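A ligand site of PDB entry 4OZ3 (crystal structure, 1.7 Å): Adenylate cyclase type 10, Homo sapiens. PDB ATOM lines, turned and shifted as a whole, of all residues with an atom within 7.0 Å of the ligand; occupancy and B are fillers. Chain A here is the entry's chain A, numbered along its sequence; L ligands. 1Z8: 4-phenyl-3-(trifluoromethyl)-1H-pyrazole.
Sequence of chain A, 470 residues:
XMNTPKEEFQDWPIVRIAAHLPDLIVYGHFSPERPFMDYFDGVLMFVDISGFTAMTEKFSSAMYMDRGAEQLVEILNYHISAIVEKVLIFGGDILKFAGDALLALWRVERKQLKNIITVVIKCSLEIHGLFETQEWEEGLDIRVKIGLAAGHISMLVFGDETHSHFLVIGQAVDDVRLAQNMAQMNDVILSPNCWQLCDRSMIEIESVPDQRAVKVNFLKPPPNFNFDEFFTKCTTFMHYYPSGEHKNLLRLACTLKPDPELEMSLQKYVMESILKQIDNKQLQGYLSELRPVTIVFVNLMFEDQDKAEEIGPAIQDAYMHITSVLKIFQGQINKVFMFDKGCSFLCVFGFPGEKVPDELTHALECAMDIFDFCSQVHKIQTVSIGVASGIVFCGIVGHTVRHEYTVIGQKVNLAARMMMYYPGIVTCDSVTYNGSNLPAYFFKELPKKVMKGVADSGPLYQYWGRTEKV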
ATOM      1  N   PHE A  46      27.631  14.454  -6.444  1.00  0.00           N
ATOM      2  CA  PHE A  46      26.793  13.680  -5.516  1.00  0.00           C
ATOM      3  C   PHE A  46      27.195  12.226  -5.640  1.00  0.00           C
ATOM      4  O   PHE A  46      27.043  11.625  -6.711  1.00  0.00           O
ATOM      5  CB  PHE A  46      25.307  13.893  -5.874  1.00  0.00           C
ATOM      6  CG  PHE A  46      24.271  13.675  -4.798  1.00  0.00           C
ATOM      7  CD1 PHE A  46      24.435  14.234  -3.531  1.00  0.00           C
ATOM      8  CD2 PHE A  46      23.111  12.961  -5.053  1.00  0.00           C
ATOM      9  CE1 PHE A  46      23.477  14.054  -2.543  1.00  0.00           C
ATOM     10  CE2 PHE A  46      22.152  12.779  -4.050  1.00  0.00           C
ATOM     11  CZ  PHE A  46      22.333  13.333  -2.812  1.00  0.00           C
ATOM     12  N   LEU A  95      30.397  18.935   1.446  1.00  0.00           N
ATOM     13  CA  LEU A  95      29.352  19.738   2.110  1.00  0.00           C
ATOM     14  C   LEU A  95      28.625  19.001   3.212  1.00  0.00           C
ATOM     15  O   LEU A  95      28.436  19.566   4.291  1.00  0.00           O
ATOM     16  CB  LEU A  95      28.316  20.208   1.100  1.00  0.00           C
ATOM     17  CG  LEU A  95      28.837  21.219   0.076  1.00  0.00           C
ATOM     18  CD1 LEU A  95      27.702  21.752  -0.788  1.00  0.00           C
ATOM     19  CD2 LEU A  95      29.656  22.332   0.779  1.00  0.00           C
ATOM     20  N   LYS A  96      28.192  17.784   2.920  1.00  0.00           N
ATOM     21  CA  LYS A  96      27.338  17.049   3.853  1.00  0.00           C
ATOM     22  C   LYS A  96      27.346  15.570   3.534  1.00  0.00           C
ATOM     23  O   LYS A  96      27.503  15.179   2.373  1.00  0.00           O
ATOM     24  CB  LYS A  96      25.873  17.569   3.729  1.00  0.00           C
ATOM     25  CG  LYS A  96      25.179  17.419   5.090  1.00  0.00           C
ATOM     26  CD  LYS A  96      23.925  18.250   5.223  1.00  0.00           C
ATOM     27  CE  LYS A  96      24.133  19.736   5.426  1.00  0.00           C
ATOM     28  NZ  LYS A  96      22.794  20.394   5.609  1.00  0.00           N
ATOM     29  N   PHE A  97      27.179  14.760   4.599  1.00  0.00           N
ATOM     30  CA  PHE A  97      26.912  13.338   4.482  1.00  0.00           C
ATOM     31  C   PHE A  97      25.437  13.120   4.837  1.00  0.00           C
ATOM     32  O   PHE A  97      24.910  13.670   5.805  1.00  0.00           O
ATOM     33  CB  PHE A  97      27.771  12.525   5.505  1.00  0.00           C
ATOM     34  CG  PHE A  97      29.267  12.653   5.331  1.00  0.00           C
ATOM     35  CD1 PHE A  97      29.959  13.737   5.874  1.00  0.00           C
ATOM     36  CD2 PHE A  97      29.993  11.692   4.627  1.00  0.00           C
ATOM     37  CE1 PHE A  97      31.361  13.857   5.727  1.00  0.00           C
ATOM     38  CE2 PHE A  97      31.382  11.812   4.478  1.00  0.00           C
ATOM     39  CZ  PHE A  97      32.065  12.895   5.028  1.00  0.00           C
ATOM     40  N   ALA A  98      24.784  12.304   4.032  1.00  0.00           N
ATOM     41  CA  ALA A  98      23.553  11.634   4.476  1.00  0.00           C
ATOM     42  C   ALA A  98      23.839  10.100   4.560  1.00  0.00           C
ATOM     43  O   ALA A  98      24.923   9.651   4.160  1.00  0.00           O
ATOM     44  CB  ALA A  98      22.427  11.946   3.482  1.00  0.00           C
ATOM     45  N   GLY A  99      22.873   9.335   5.097  1.00  0.00           N
ATOM     46  CA  GLY A  99      22.920   7.871   5.129  1.00  0.00           C
ATOM     47  C   GLY A  99      22.456   7.234   3.831  1.00  0.00           C
ATOM     48  O   GLY A  99      21.657   6.272   3.817  1.00  0.00           O
ATOM     49  N   ASP A 100      22.968   7.803   2.718  1.00  0.00           N
ATOM     50  CA  ASP A 100      22.703   7.441   1.339  1.00  0.00           C
ATOM     51  C   ASP A 100      23.711   8.190   0.422  1.00  0.00           C
ATOM     52  O   ASP A 100      24.009   7.662  -0.613  1.00  0.00           O
ATOM     53  CB  ASP A 100      21.272   7.813   0.956  1.00  0.00           C
ATOM     54  CG  ASP A 100      21.030   9.313   1.028  1.00  0.00           C
ATOM     55  OD1 ASP A 100      21.059   9.975  -0.031  1.00  0.00           O
ATOM     56  OD2 ASP A 100      20.887   9.832   2.154  1.00  0.00           O
ATOM     57  N   ALA A 101      24.223   9.407   0.792  1.00  0.00           N
ATOM     58  CA  ALA A 101      25.040  10.191  -0.143  1.00  0.00           C
ATOM     59  C   ALA A 101      26.036  11.134   0.532  1.00  0.00           C
ATOM     60  O   ALA A 101      25.888  11.507   1.683  1.00  0.00           O
ATOM     61  CB  ALA A 101      24.154  10.992  -1.092  1.00  0.00           C
ATOM     62  N   LEU A 102      27.053  11.523  -0.229  1.00  0.00           N
ATOM     63  CA  LEU A 102      28.015  12.550   0.169  1.00  0.00           C
ATOM     64  C   LEU A 102      27.818  13.597  -0.938  1.00  0.00           C
ATOM     65  O   LEU A 102      27.769  13.229  -2.105  1.00  0.00           O
ATOM     66  CB  LEU A 102      29.401  11.843   0.112  1.00  0.00           C
ATOM     67  CG  LEU A 102      30.693  12.533   0.238  1.00  0.00           C
ATOM     68  CD1 LEU A 102      31.764  11.506   0.697  1.00  0.00           C
ATOM     69  CD2 LEU A 102      31.127  13.107  -1.111  1.00  0.00           C
ATOM     70  N   LEU A 103      27.698  14.873  -0.590  1.00  0.00           N
ATOM     71  CA  LEU A 103      27.671  15.921  -1.604  1.00  0.00           C
ATOM     72  C   LEU A 103      28.925  16.742  -1.481  1.00  0.00           C
ATOM     73  O   LEU A 103      29.240  17.178  -0.359  1.00  0.00           O
ATOM     74  CB  LEU A 103      26.459  16.822  -1.326  1.00  0.00           C
ATOM     75  CG  LEU A 103      26.276  18.039  -2.238  1.00  0.00           C
ATOM     76  CD1 LEU A 103      25.984  17.586  -3.685  1.00  0.00           C
ATOM     77  CD2 LEU A 103      25.092  18.920  -1.710  1.00  0.00           C
ATOM     78  N   ALA A 104      29.645  16.943  -2.594  1.00  0.00           N
ATOM     79  CA  ALA A 104      30.869  17.774  -2.537  1.00  0.00           C
ATOM     80  C   ALA A 104      30.723  18.945  -3.526  1.00  0.00           C
ATOM     81  O   ALA A 104      30.015  18.841  -4.547  1.00  0.00           O
ATOM     82  CB  ALA A 104      32.100  16.937  -2.889  1.00  0.00           C
ATOM     83  N   LEU A 156      21.842  28.675   1.895  1.00  0.00           N
ATOM     84  CA  LEU A 156      20.958  29.227   2.891  1.00  0.00           C
ATOM     85  C   LEU A 156      21.507  28.813   4.242  1.00  0.00           C
ATOM     86  O   LEU A 156      21.789  27.637   4.429  1.00  0.00           O
ATOM     87  CB  LEU A 156      19.532  28.631   2.719  1.00  0.00           C
ATOM     88  CG  LEU A 156      18.607  28.913   3.925  1.00  0.00           C
ATOM     89  CD1 LEU A 156      18.358  30.443   4.059  1.00  0.00           C
ATOM     90  CD2 LEU A 156      17.283  28.208   3.758  1.00  0.00           C
ATOM     91  N   PHE A 166      22.813  24.728   7.439  1.00  0.00           N
ATOM     92  CA  PHE A 166      22.883  25.275   6.105  1.00  0.00           C
ATOM     93  C   PHE A 166      22.355  24.257   5.076  1.00  0.00           C
ATOM     94  O   PHE A 166      22.282  23.043   5.348  1.00  0.00           O
ATOM     95  CB  PHE A 166      24.316  25.733   5.765  1.00  0.00           C
ATOM     96  CG  PHE A 166      25.181  24.573   5.313  1.00  0.00           C
ATOM     97  CD1 PHE A 166      25.330  24.285   3.961  1.00  0.00           C
ATOM     98  CD2 PHE A 166      25.820  23.766   6.247  1.00  0.00           C
ATOM     99  CE1 PHE A 166      26.120  23.188   3.542  1.00  0.00           C
ATOM    100  CE2 PHE A 166      26.609  22.679   5.830  1.00  0.00           C
ATOM    101  CZ  PHE A 166      26.750  22.408   4.487  1.00  0.00           C
ATOM    102  N   LEU A 167      22.029  24.762   3.902  1.00  0.00           N
ATOM    103  CA  LEU A 167      21.562  24.022   2.738  1.00  0.00           C
ATOM    104  C   LEU A 167      22.095  24.701   1.516  1.00  0.00           C
ATOM    105  O   LEU A 167      22.271  25.925   1.513  1.00  0.00           O
ATOM    106  CB  LEU A 167      20.022  24.186   2.605  1.00  0.00           C
ATOM    107  CG  LEU A 167      19.147  23.564   3.584  1.00  0.00           C
ATOM    108  CD1 LEU A 167      17.742  24.042   3.364  1.00  0.00           C
ATOM    109  CD2 LEU A 167      19.205  22.092   3.421  1.00  0.00           C
ATOM    110  N   VAL A 168      22.372  23.931   0.467  1.00  0.00           N
ATOM    111  CA  VAL A 168      22.586  24.569  -0.832  1.00  0.00           C
ATOM    112  C   VAL A 168      21.347  24.239  -1.655  1.00  0.00           C
ATOM    113  O   VAL A 168      20.735  23.165  -1.499  1.00  0.00           O
ATOM    114  CB  VAL A 168      23.883  24.141  -1.555  1.00  0.00           C
ATOM    115  CG1 VAL A 168      25.101  24.790  -0.896  1.00  0.00           C
ATOM    116  CG2 VAL A 168      24.029  22.609  -1.642  1.00  0.00           C
ATOM    117  N   ILE A 169      20.961  25.188  -2.522  1.00  0.00           N
ATOM    118  CA  ILE A 169      19.733  25.083  -3.285  1.00  0.00           C
ATOM    119  C   ILE A 169      19.945  25.616  -4.689  1.00  0.00           C
ATOM    120  O   ILE A 169      20.975  26.236  -4.942  1.00  0.00           O
ATOM    121  CB  ILE A 169      18.529  25.757  -2.556  1.00  0.00           C
ATOM    122  CG1 ILE A 169      18.567  27.260  -2.681  1.00  0.00           C
ATOM    123  CG2 ILE A 169      18.390  25.384  -1.061  1.00  0.00           C
ATOM    124  CD1 ILE A 169      17.227  27.853  -2.480  1.00  0.00           C
ATOM    125  N   VAL A 173      21.788  22.177  -7.814  1.00  0.00           N
ATOM    126  CA  VAL A 173      21.534  21.244  -6.704  1.00  0.00           C
ATOM    127  C   VAL A 173      20.446  20.223  -7.113  1.00  0.00           C
ATOM    128  O   VAL A 173      20.636  19.022  -6.917  1.00  0.00           O
ATOM    129  CB  VAL A 173      21.159  22.022  -5.425  1.00  0.00           C
ATOM    130  CG1 VAL A 173      20.699  21.081  -4.313  1.00  0.00           C
ATOM    131  CG2 VAL A 173      22.371  22.870  -4.920  1.00  0.00           C
ATOM    132  N   ASP A 174      19.355  20.697  -7.666  1.00  0.00           N
ATOM    133  CA  ASP A 174      18.288  19.808  -8.194  1.00  0.00           C
ATOM    134  C   ASP A 174      18.895  18.847  -9.232  1.00  0.00           C
ATOM    135  O   ASP A 174      18.690  17.649  -9.149  1.00  0.00           O
ATOM    136  CB  ASP A 174      17.188  20.662  -8.836  1.00  0.00           C
ATOM    137  CG  ASP A 174      16.546  21.658  -7.896  1.00  0.00           C
ATOM    138  OD1 ASP A 174      16.730  21.503  -6.662  1.00  0.00           O
ATOM    139  OD2 ASP A 174      15.878  22.584  -8.381  1.00  0.00           O
ATOM    140  N   VAL A 176      21.995  17.799  -9.697  1.00  0.00           N
ATOM    141  CA  VAL A 176      22.926  16.780  -9.263  1.00  0.00           C
ATOM    142  C   VAL A 176      22.195  15.585  -8.706  1.00  0.00           C
ATOM    143  O   VAL A 176      22.677  14.462  -8.853  1.00  0.00           O
ATOM    144  CB  VAL A 176      24.020  17.337  -8.313  1.00  0.00           C
ATOM    145  CG1 VAL A 176      23.511  17.475  -6.873  1.00  0.00           C
ATOM    146  CG2 VAL A 176      25.276  16.508  -8.395  1.00  0.00           C
ATOM    147  N   ARG A 177      21.045  15.839  -8.063  1.00  0.00           N
ATOM    148  CA  ARG A 177      20.149  14.813  -7.528  1.00  0.00           C
ATOM    149  C   ARG A 177      19.601  13.992  -8.713  1.00  0.00           C
ATOM    150  O   ARG A 177      19.701  12.766  -8.695  1.00  0.00           O
ATOM    151  CB  ARG A 177      18.999  15.474  -6.767  1.00  0.00           C
ATOM    152  CG  ARG A 177      17.930  14.500  -6.224  1.00  0.00           C
ATOM    153  CD  ARG A 177      18.386  13.645  -5.047  1.00  0.00           C
ATOM    154  NE  ARG A 177      18.475  14.429  -3.807  1.00  0.00           N
ATOM    155  CZ  ARG A 177      18.785  13.931  -2.619  1.00  0.00           C
ATOM    156  NH1 ARG A 177      19.018  12.628  -2.473  1.00  0.00           N
ATOM    157  NH2 ARG A 177      18.842  14.713  -1.562  1.00  0.00           N
ATOM    158  N   LYS A 335      19.703  16.142  10.120  1.00  0.00           N
ATOM    159  CA  LYS A 335      20.088  16.620   8.787  1.00  0.00           C
ATOM    160  C   LYS A 335      18.972  17.445   8.247  1.00  0.00           C
ATOM    161  O   LYS A 335      17.803  17.169   8.533  1.00  0.00           O
ATOM    162  CB  LYS A 335      20.267  15.469   7.746  1.00  0.00           C
ATOM    163  CG  LYS A 335      21.324  14.399   7.973  1.00  0.00           C
ATOM    164  CD  LYS A 335      22.759  14.931   7.984  1.00  0.00           C
ATOM    165  CE  LYS A 335      23.635  13.895   8.633  1.00  0.00           C
ATOM    166  NZ  LYS A 335      25.036  14.334   8.647  1.00  0.00           N
ATOM    167  N   VAL A 336      19.334  18.447   7.425  1.00  0.00           N
ATOM    168  CA  VAL A 336      18.387  19.131   6.552  1.00  0.00           C
ATOM    169  C   VAL A 336      19.042  19.127   5.190  1.00  0.00           C
ATOM    170  O   VAL A 336      20.254  19.315   5.081  1.00  0.00           O
ATOM    171  CB  VAL A 336      18.097  20.597   7.004  1.00  0.00           C
ATOM    172  CG1 VAL A 336      16.913  21.179   6.266  1.00  0.00           C
ATOM    173  CG2 VAL A 336      17.867  20.706   8.506  1.00  0.00           C
ATOM    174  N   PHE A 337      18.252  18.911   4.158  1.00  0.00           N
ATOM    175  CA  PHE A 337      18.729  18.963   2.783  1.00  0.00           C
ATOM    176  C   PHE A 337      17.580  19.153   1.846  1.00  0.00           C
ATOM    177  O   PHE A 337      16.418  18.998   2.260  1.00  0.00           O
ATOM    178  CB  PHE A 337      19.495  17.659   2.449  1.00  0.00           C
ATOM    179  CG  PHE A 337      18.703  16.403   2.682  1.00  0.00           C
ATOM    180  CD1 PHE A 337      17.837  15.911   1.704  1.00  0.00           C
ATOM    181  CD2 PHE A 337      18.804  15.713   3.877  1.00  0.00           C
ATOM    182  CE1 PHE A 337      17.094  14.740   1.919  1.00  0.00           C
ATOM    183  CE2 PHE A 337      18.068  14.542   4.099  1.00  0.00           C
ATOM    184  CZ  PHE A 337      17.223  14.061   3.119  1.00  0.00           C
ATOM    185  N   MET A 338      17.922  19.458   0.566  1.00  0.00           N
ATOM    186  CA  MET A 338      16.963  19.481  -0.541  1.00  0.00           C
ATOM    187  C   MET A 338      16.745  18.089  -1.132  1.00  0.00           C
ATOM    188  O   MET A 338      17.714  17.354  -1.366  1.00  0.00           O
ATOM    189  CB  MET A 338      17.407  20.461  -1.648  1.00  0.00           C
ATOM    190  CG  MET A 338      17.570  21.901  -1.177  1.00  0.00           C
ATOM    191  SD  MET A 338      16.327  22.479   0.008  1.00  0.00           S
ATOM    192  CE  MET A 338      15.190  23.249  -1.061  1.00  0.00           C
ATOM    193  N   PHE A 339      15.463  17.714  -1.384  1.00  0.00           N
ATOM    194  CA  PHE A 339      15.080  16.519  -2.164  1.00  0.00           C
ATOM    195  C   PHE A 339      13.945  16.920  -3.086  1.00  0.00           C
ATOM    196  O   PHE A 339      12.863  17.263  -2.596  1.00  0.00           O
ATOM    197  CB  PHE A 339      14.639  15.330  -1.272  1.00  0.00           C
ATOM    198  CG  PHE A 339      14.596  14.011  -2.015  1.00  0.00           C
ATOM    199  CD1 PHE A 339      15.614  13.062  -1.857  1.00  0.00           C
ATOM    200  CD2 PHE A 339      13.537  13.704  -2.869  1.00  0.00           C
ATOM    201  CE1 PHE A 339      15.571  11.845  -2.547  1.00  0.00           C
ATOM    202  CE2 PHE A 339      13.502  12.488  -3.566  1.00  0.00           C
ATOM    203  CZ  PHE A 339      14.511  11.567  -3.397  1.00  0.00           C
HETATM  204  C2  1Z8 L   1      23.024  20.018   1.723  1.00  0.00           C
HETATM  205  C5  1Z8 L   1      22.123  19.784   0.585  1.00  0.00           C
HETATM  206  C10 1Z8 L   1      21.777  18.597  -0.054  1.00  0.00           C
HETATM  207  C11 1Z8 L   1      22.195  17.205   0.187  1.00  0.00           C
HETATM  208  C12 1Z8 L   1      21.319  16.155  -0.050  1.00  0.00           C
HETATM  209  C13 1Z8 L   1      21.692  14.852   0.187  1.00  0.00           C
HETATM  210  C14 1Z8 L   1      22.948  14.568   0.679  1.00  0.00           C
HETATM  211  C15 1Z8 L   1      23.829  15.595   0.934  1.00  0.00           C
HETATM  212  C16 1Z8 L   1      23.456  16.907   0.698  1.00  0.00           C
HETATM  213  F1  1Z8 L   1      22.912  21.197   2.170  1.00  0.00           F
HETATM  214  F3  1Z8 L   1      24.305  19.865   1.418  1.00  0.00           F
HETATM  215  F4  1Z8 L   1      22.780  19.209   2.761  1.00  0.00           F
HETATM  216  N6  1Z8 L   1      21.505  20.839   0.061  1.00  0.00           N
HETATM  217  N7  1Z8 L   1      20.769  20.325  -0.937  1.00  0.00           N
HETATM  218  C9  1Z8 L   1      20.897  18.988  -1.036  1.00  0.00           C
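A nitrogen (N7) of the ligand sits at hydrogen-bond distance from the backbone carbonyl oxygen of Val 168.
The backbone NH (N) of Met 338 sits close to a nitrogen (N7) of the ligand, 3.3 Å away.
N of Val 168 is in hydrogen-bond range of N6 of the ligand, at 3.2 Å.
The backbone carbonyl oxygen (O) of Leu 167 is in hydrogen-bond range of the backbone NH (N) of Leu 156 (2.8 Å).
O of Met 338 sits at hydrogen-bond distance from NH2 of Arg 177.
The backbone carbonyl oxygen (O) of Phe 166 lies within hydrogen-bond range of the side-chain amino group (NZ) of Lys 96 (2.7 Å).
The backbone NH of Leu 103 lies within hydrogen-bond range of the backbone carbonyl oxygen of Lys 96 (3.0 Å).
The side-chain amino group (NZ) of Lys 96 lies within hydrogen-bond range of the backbone carbonyl oxygen (O) of Val 336, 2.8 Å away.
The backbone NH (N) of Leu 95 lies within hydrogen-bond range of the backbone carbonyl oxygen (O) of Leu 103.
The side-chain amino group (NZ) of Lys 96 sits close to a fluorine (F4) of the ligand.
The backbone carbonyl oxygen (O) of Val 336 sits close to a fluorine (F4) of the ligand (3.4 Å).
Phe 46 touches the ligand.
Ala 98 touches the ligand.
Leu 103 touches the ligand (CD2 to F3, 3.4 Å).
Phe 166 touches the ligand.
Leu 167 touches the ligand (CA to F1, 3.2 Å).
Val 173 touches the ligand.
Arg 177 touches the ligand.
Phe 337 touches the ligand (CB to C12, 3.4 Å).
Hydrophobic or aromatic side chains within 4 Å of the ligand: Phe 46, Ala 98, Leu 103, Val 168, Val 173, Phe 337 and Met 338.
12 residues have an atom within 4 Å of the ligand: Phe 46, Lys 96, Ala 98, Leu 103, Phe 166, Leu 167, Val 168, Val 173, Arg 177, Val 336, Phe 337 and Met 338.
The nearest printed residue that does not touch the ligand is Leu 95 (4.04 Å).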
